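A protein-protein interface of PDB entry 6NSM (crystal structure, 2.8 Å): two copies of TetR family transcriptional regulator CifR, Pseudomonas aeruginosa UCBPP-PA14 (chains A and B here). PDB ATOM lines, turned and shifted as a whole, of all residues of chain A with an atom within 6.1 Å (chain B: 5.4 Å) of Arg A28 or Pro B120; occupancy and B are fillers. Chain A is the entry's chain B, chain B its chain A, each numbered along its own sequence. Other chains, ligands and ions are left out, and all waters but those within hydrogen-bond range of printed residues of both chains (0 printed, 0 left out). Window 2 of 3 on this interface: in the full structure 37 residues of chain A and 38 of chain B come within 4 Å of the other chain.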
ATOM      1  N   ASP A  23      23.324 -32.048   2.139  1.00  0.00           N
ATOM      2  CA  ASP A  23      23.445 -32.044   3.594  1.00  0.00           C
ATOM      3  C   ASP A  23      22.599 -30.938   4.212  1.00  0.00           C
ATOM      4  O   ASP A  23      21.943 -31.149   5.239  1.00  0.00           O
ATOM      5  CB  ASP A  23      24.911 -31.891   3.997  1.00  0.00           C
ATOM      6  CG  ASP A  23      25.673 -33.202   3.937  1.00  0.00           C
ATOM      7  OD1 ASP A  23      25.034 -34.255   3.728  1.00  0.00           O
ATOM      8  OD2 ASP A  23      26.912 -33.179   4.099  1.00  0.00           O
ATOM      9  N   VAL A  24      22.614 -29.747   3.610  1.00  0.00           N
ATOM     10  CA  VAL A  24      21.856 -28.625   4.161  1.00  0.00           C
ATOM     11  C   VAL A  24      20.362 -28.925   4.122  1.00  0.00           C
ATOM     12  O   VAL A  24      19.641 -28.711   5.104  1.00  0.00           O
ATOM     13  CB  VAL A  24      22.207 -27.320   3.423  1.00  0.00           C
ATOM     14  CG1 VAL A  24      21.088 -26.304   3.568  1.00  0.00           C
ATOM     15  CG2 VAL A  24      23.519 -26.755   3.942  1.00  0.00           C
ATOM     16  N   PHE A  25      19.874 -29.417   2.977  1.00  0.00           N
ATOM     17  CA  PHE A  25      18.495 -29.892   2.897  1.00  0.00           C
ATOM     18  C   PHE A  25      18.215 -30.953   3.956  1.00  0.00           C
ATOM     19  O   PHE A  25      17.145 -30.960   4.573  1.00  0.00           O
ATOM     20  CB  PHE A  25      18.207 -30.453   1.504  1.00  0.00           C
ATOM     21  CG  PHE A  25      18.083 -29.406   0.435  1.00  0.00           C
ATOM     22  CD1 PHE A  25      17.294 -28.285   0.632  1.00  0.00           C
ATOM     23  CD2 PHE A  25      18.743 -29.550  -0.775  1.00  0.00           C
ATOM     24  CE1 PHE A  25      17.173 -27.323  -0.353  1.00  0.00           C
ATOM     25  CE2 PHE A  25      18.627 -28.590  -1.764  1.00  0.00           C
ATOM     26  CZ  PHE A  25      17.841 -27.476  -1.552  1.00  0.00           C
ATOM     27  N   TRP A  26      19.168 -31.864   4.167  1.00  0.00           N
ATOM     28  CA  TRP A  26      18.971 -32.965   5.105  1.00  0.00           C
ATOM     29  C   TRP A  26      18.712 -32.461   6.521  1.00  0.00           C
ATOM     30  O   TRP A  26      18.026 -33.129   7.303  1.00  0.00           O
ATOM     31  CB  TRP A  26      20.191 -33.887   5.070  1.00  0.00           C
ATOM     32  CG  TRP A  26      19.928 -35.300   5.502  1.00  0.00           C
ATOM     33  CD1 TRP A  26      18.914 -35.744   6.298  1.00  0.00           C
ATOM     34  CD2 TRP A  26      20.695 -36.457   5.148  1.00  0.00           C
ATOM     35  NE1 TRP A  26      19.005 -37.104   6.467  1.00  0.00           N
ATOM     36  CE2 TRP A  26      20.090 -37.566   5.770  1.00  0.00           C
ATOM     37  CE3 TRP A  26      21.837 -36.662   4.367  1.00  0.00           C
ATOM     38  CZ2 TRP A  26      20.587 -38.860   5.636  1.00  0.00           C
ATOM     39  CZ3 TRP A  26      22.329 -37.948   4.235  1.00  0.00           C
ATOM     40  CH2 TRP A  26      21.704 -39.031   4.866  1.00  0.00           C
ATOM     41  N   VAL A  27      19.230 -31.286   6.861  1.00  0.00           N
ATOM     42  CA  VAL A  27      19.149 -30.761   8.217  1.00  0.00           C
ATOM     43  C   VAL A  27      18.097 -29.667   8.343  1.00  0.00           C
ATOM     44  O   VAL A  27      17.337 -29.645   9.313  1.00  0.00           O
ATOM     45  CB  VAL A  27      20.535 -30.271   8.692  1.00  0.00           C
ATOM     46  CG1 VAL A  27      20.419 -29.508  10.003  1.00  0.00           C
ATOM     47  CG2 VAL A  27      21.491 -31.444   8.836  1.00  0.00           C
ATOM     48  N   ARG A  28      18.031 -28.752   7.377  1.00  0.00           N
ATOM     49  CA  ARG A  28      17.087 -27.643   7.435  1.00  0.00           C
ATOM     50  C   ARG A  28      15.807 -27.886   6.646  1.00  0.00           C
ATOM     51  O   ARG A  28      14.846 -27.129   6.814  1.00  0.00           O
ATOM     52  CB  ARG A  28      17.746 -26.350   6.937  1.00  0.00           C
ATOM     53  CG  ARG A  28      19.004 -25.951   7.689  1.00  0.00           C
ATOM     54  CD  ARG A  28      19.747 -24.855   6.943  1.00  0.00           C
ATOM     55  NE  ARG A  28      20.606 -24.070   7.822  1.00  0.00           N
ATOM     56  CZ  ARG A  28      20.679 -22.747   7.809  1.00  0.00           C
ATOM     57  NH1 ARG A  28      19.937 -22.021   6.989  1.00  0.00           N
ATOM     58  NH2 ARG A  28      21.517 -22.135   8.642  1.00  0.00           N
ATOM     59  N   GLY A  29      15.761 -28.911   5.800  1.00  0.00           N
ATOM     60  CA  GLY A  29      14.611 -29.141   4.953  1.00  0.00           C
ATOM     61  C   GLY A  29      14.651 -28.278   3.706  1.00  0.00           C
ATOM     62  O   GLY A  29      15.497 -27.397   3.540  1.00  0.00           O
ATOM     63  N   TYR A  30      13.709 -28.549   2.800  1.00  0.00           N
ATOM     64  CA  TYR A  30      13.678 -27.833   1.527  1.00  0.00           C
ATOM     65  C   TYR A  30      13.434 -26.337   1.692  1.00  0.00           C
ATOM     66  O   TYR A  30      14.234 -25.511   1.239  1.00  0.00           O
ATOM     67  CB  TYR A  30      12.602 -28.423   0.615  1.00  0.00           C
ATOM     68  CG  TYR A  30      12.391 -27.629  -0.654  1.00  0.00           C
ATOM     69  CD1 TYR A  30      13.395 -27.536  -1.610  1.00  0.00           C
ATOM     70  CD2 TYR A  30      11.195 -26.964  -0.893  1.00  0.00           C
ATOM     71  CE1 TYR A  30      13.212 -26.810  -2.772  1.00  0.00           C
ATOM     72  CE2 TYR A  30      11.004 -26.233  -2.051  1.00  0.00           C
ATOM     73  CZ  TYR A  30      12.015 -26.160  -2.986  1.00  0.00           C
ATOM     74  OH  TYR A  30      11.828 -25.437  -4.141  1.00  0.00           O
ATOM     75  N   GLU A  31      12.329 -25.968   2.345  1.00  0.00           N
ATOM     76  CA  GLU A  31      12.022 -24.551   2.517  1.00  0.00           C
ATOM     77  C   GLU A  31      12.905 -23.945   3.600  1.00  0.00           C
ATOM     78  O   GLU A  31      13.192 -22.743   3.561  1.00  0.00           O
ATOM     79  CB  GLU A  31      10.549 -24.344   2.867  1.00  0.00           C
ATOM     80  CG  GLU A  31       9.572 -24.773   1.787  1.00  0.00           C
ATOM     81  CD  GLU A  31       8.146 -24.368   2.107  1.00  0.00           C
ATOM     82  OE1 GLU A  31       7.766 -24.415   3.297  1.00  0.00           O
ATOM     83  OE2 GLU A  31       7.405 -23.998   1.172  1.00  0.00           O
ATOM     84  N   GLY A  32      13.345 -24.749   4.566  1.00  0.00           N
ATOM     85  CA  GLY A  32      14.232 -24.246   5.598  1.00  0.00           C
ATOM     86  C   GLY A  32      15.635 -23.932   5.125  1.00  0.00           C
ATOM     87  O   GLY A  32      16.391 -23.301   5.873  1.00  0.00           O
ATOM     88  N   ALA A  33      15.997 -24.346   3.914  1.00  0.00           N
ATOM     89  CA  ALA A  33      17.337 -24.119   3.386  1.00  0.00           C
ATOM     90  C   ALA A  33      17.320 -22.849   2.545  1.00  0.00           C
ATOM     91  O   ALA A  33      16.798 -22.842   1.425  1.00  0.00           O
ATOM     92  CB  ALA A  33      17.783 -25.313   2.549  1.00  0.00           C
ATOM     93  N   SER A  34      17.892 -21.776   3.082  1.00  0.00           N
ATOM     94  CA  SER A  34      18.043 -20.544   2.331  1.00  0.00           C
ATOM     95  C   SER A  34      19.216 -20.657   1.364  1.00  0.00           C
ATOM     96  O   SER A  34      20.147 -21.441   1.564  1.00  0.00           O
ATOM     97  CB  SER A  34      18.272 -19.367   3.277  1.00  0.00           C
ATOM     98  OG  SER A  34      19.492 -19.510   3.981  1.00  0.00           O
ATOM     99  N   ALA A  37      22.532 -20.042   3.166  1.00  0.00           N
ATOM    100  CA  ALA A  37      23.137 -21.212   3.794  1.00  0.00           C
ATOM    101  C   ALA A  37      23.629 -22.203   2.748  1.00  0.00           C
ATOM    102  O   ALA A  37      24.667 -22.844   2.945  1.00  0.00           O
ATOM    103  CB  ALA A  37      22.151 -21.863   4.760  1.00  0.00           C
ATOM    104  N   ALA A 114      12.516 -33.893   5.031  1.00  0.00           N
ATOM    105  CA  ALA A 114      12.851 -32.665   4.313  1.00  0.00           C
ATOM    106  C   ALA A 114      11.634 -31.779   4.065  1.00  0.00           C
ATOM    107  O   ALA A 114      11.758 -30.549   4.089  1.00  0.00           O
ATOM    108  CB  ALA A 114      13.557 -32.983   2.995  1.00  0.00           C
ATOM    109  N   LYS A 178      15.861 -38.437  14.726  1.00  0.00           N
ATOM    110  CA  LYS A 178      15.973 -36.990  14.876  1.00  0.00           C
ATOM    111  C   LYS A 178      15.807 -36.586  16.333  1.00  0.00           C
ATOM    112  O   LYS A 178      16.475 -35.663  16.815  1.00  0.00           O
ATOM    113  CB  LYS A 178      14.941 -36.287  13.995  1.00  0.00           C
ATOM    114  CG  LYS A 178      14.930 -34.776  14.122  1.00  0.00           C
ATOM    115  CD  LYS A 178      15.613 -34.124  12.930  1.00  0.00           C
ATOM    116  CE  LYS A 178      16.408 -32.904  13.344  1.00  0.00           C
ATOM    117  NZ  LYS A 178      16.827 -32.091  12.172  1.00  0.00           N
ATOM    118  N   THR B 117      12.178 -30.336  10.647  1.00  0.00           N
ATOM    119  CA  THR B 117      13.394 -29.644  10.256  1.00  0.00           C
ATOM    120  C   THR B 117      13.051 -28.187   9.974  1.00  0.00           C
ATOM    121  O   THR B 117      11.881 -27.819   9.835  1.00  0.00           O
ATOM    122  CB  THR B 117      14.021 -30.289   9.013  1.00  0.00           C
ATOM    123  OG1 THR B 117      12.988 -30.632   8.081  1.00  0.00           O
ATOM    124  CG2 THR B 117      14.776 -31.552   9.397  1.00  0.00           C
ATOM    125  N   GLY B 118      14.078 -27.352   9.889  1.00  0.00           N
ATOM    126  CA  GLY B 118      13.861 -25.953   9.583  1.00  0.00           C
ATOM    127  C   GLY B 118      15.116 -25.138   9.819  1.00  0.00           C
ATOM    128  O   GLY B 118      16.204 -25.679  10.034  1.00  0.00           O
ATOM    129  N   THR B 119      14.934 -23.819   9.767  1.00  0.00           N
ATOM    130  CA  THR B 119      16.028 -22.888   9.974  1.00  0.00           C
ATOM    131  C   THR B 119      16.548 -22.986  11.407  1.00  0.00           C
ATOM    132  O   THR B 119      15.822 -23.401  12.314  1.00  0.00           O
ATOM    133  CB  THR B 119      15.556 -21.463   9.698  1.00  0.00           C
ATOM    134  OG1 THR B 119      14.528 -21.109  10.633  1.00  0.00           O
ATOM    135  CG2 THR B 119      15.005 -21.350   8.285  1.00  0.00           C
ATOM    136  N   PRO B 120      17.809 -22.610  11.636  1.00  0.00           N
ATOM    137  CA  PRO B 120      18.313 -22.551  13.019  1.00  0.00           C
ATOM    138  C   PRO B 120      17.552 -21.582  13.908  1.00  0.00           C
ATOM    139  O   PRO B 120      17.680 -21.659  15.136  1.00  0.00           O
ATOM    140  CB  PRO B 120      19.781 -22.125  12.849  1.00  0.00           C
ATOM    141  CG  PRO B 120      19.877 -21.592  11.448  1.00  0.00           C
ATOM    142  CD  PRO B 120      18.873 -22.359  10.653  1.00  0.00           C
ATOM    143  N   GLU B 121      16.765 -20.671  13.328  1.00  0.00           N
ATOM    144  CA  GLU B 121      16.087 -19.651  14.121  1.00  0.00           C
ATOM    145  C   GLU B 121      14.989 -20.253  14.990  1.00  0.00           C
ATOM    146  O   GLU B 121      14.662 -19.699  16.046  1.00  0.00           O
ATOM    147  CB  GLU B 121      15.502 -18.557  13.219  1.00  0.00           C
ATOM    148  CG  GLU B 121      16.170 -18.331  11.846  1.00  0.00           C
ATOM    149  CD  GLU B 121      17.696 -18.328  11.857  1.00  0.00           C
ATOM    150  OE1 GLU B 121      18.306 -18.001  12.898  1.00  0.00           O
ATOM    151  OE2 GLU B 121      18.289 -18.659  10.809  1.00  0.00           O
ATOM    152  N   SER B 122      14.412 -21.377  14.567  1.00  0.00           N
ATOM    153  CA  SER B 122      13.206 -21.927  15.172  1.00  0.00           C
ATOM    154  C   SER B 122      13.473 -23.213  15.949  1.00  0.00           C
ATOM    155  O   SER B 122      12.574 -24.043  16.106  1.00  0.00           O
ATOM    156  CB  SER B 122      12.123 -22.149  14.117  1.00  0.00           C
ATOM    157  OG  SER B 122      12.609 -22.946  13.050  1.00  0.00           O
ATOM    158  N   GLU B 123      14.706 -23.399  16.430  1.00  0.00           N
ATOM    159  CA  GLU B 123      15.013 -24.596  17.209  1.00  0.00           C
ATOM    160  C   GLU B 123      14.179 -24.663  18.482  1.00  0.00           C
ATOM    161  O   GLU B 123      13.868 -25.759  18.960  1.00  0.00           O
ATOM    162  CB  GLU B 123      16.504 -24.652  17.541  1.00  0.00           C
ATOM    163  CG  GLU B 123      17.247 -25.789  16.853  1.00  0.00           C
ATOM    164  CD  GLU B 123      18.595 -26.077  17.485  1.00  0.00           C
ATOM    165  OE1 GLU B 123      19.094 -25.219  18.245  1.00  0.00           O
ATOM    166  OE2 GLU B 123      19.156 -27.162  17.223  1.00  0.00           O
ATOM    167  N   ARG B 126      11.179 -26.402  17.446  1.00  0.00           N
ATOM    168  CA  ARG B 126      11.442 -27.776  17.095  1.00  0.00           C
ATOM    169  C   ARG B 126      11.685 -28.628  18.316  1.00  0.00           C
ATOM    170  O   ARG B 126      11.293 -29.768  18.350  1.00  0.00           O
ATOM    171  CB  ARG B 126      12.613 -27.878  16.138  1.00  0.00           C
ATOM    172  CG  ARG B 126      12.326 -27.346  14.762  1.00  0.00           C
ATOM    173  CD  ARG B 126      13.315 -27.866  13.762  1.00  0.00           C
ATOM    174  NE  ARG B 126      14.636 -27.318  13.966  1.00  0.00           N
ATOM    175  CZ  ARG B 126      15.020 -26.143  13.512  1.00  0.00           C
ATOM    176  NH1 ARG B 126      14.192 -25.389  12.830  1.00  0.00           N
ATOM    177  NH2 ARG B 126      16.237 -25.721  13.736  1.00  0.00           N
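No position is printed for both chains. Of the 7 pairs that touch across the chains among the printed residues, none has its exchanged pair printed and touching as well.
The backbone NH (N) of Gly B118 lies close to the backbone carbonyl oxygen (O) of Arg A28 (3.2 Å).
Among the printed residues, pairs that only touch across the chains: Val A27 with Thr B117, Arg A28 with Thr B117, Arg A28 with Pro B120, Gly A29 with Thr B117, Gly A32 with Thr B119 and Lys A178 with Thr B117.
The guanidinium group (NH1) of Arg B126 sits close to the backbone carbonyl oxygen (O) of Gly B118, at 3.5 Å. The side-chain hydroxyl (OG) of Ser B122 is in hydrogen-bond range of the backbone carbonyl oxygen (O) of Thr B119 (3.3 Å). The backbone carbonyl oxygen (O) of Thr B119 is in hydrogen-bond range of the guanidinium group (NH1) of Arg B126 (2.6 Å).
Of the 15 printed residues of chain A, 5 touch a printed residue of chain B. Printed residues of chain B that touch a printed residue of chain A: Thr B117, Gly B118, Thr B119 and Pro B120. Hydrophobic or aromatic side chains of chain B that line the printed part of chain A: Pro B120. Among the printed residues, no Asp or Glu carboxylate lies within 4 Å of a Lys or Arg side-chain nitrogen of the other chain.
Of the printed residues of chain B, Val A27 touches Thr B117. Of the printed residues of chain B, Arg A28 touches Thr B117, Gly B118 and Pro B120. Of the printed residues of chain A, Gly B118 touches Arg A28 (3.2 Å). Printed residues of chain A within 4 Å of Thr B119: Gly A32. Pro B120 touches just one residue of chain A: Arg A28 (3.3 Å). Glu B123 touches none of the printed residues of chain A. The nearest residue of chain B that does not touch Arg A28 is Thr B119 (4.4 Å). The nearest residue of chain A that does not touch Pro B120 is Gly A32 (5.5 Å). The nearest printed residue of chain A that does not touch Gly B118 is Val A27 (4.03 Å).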
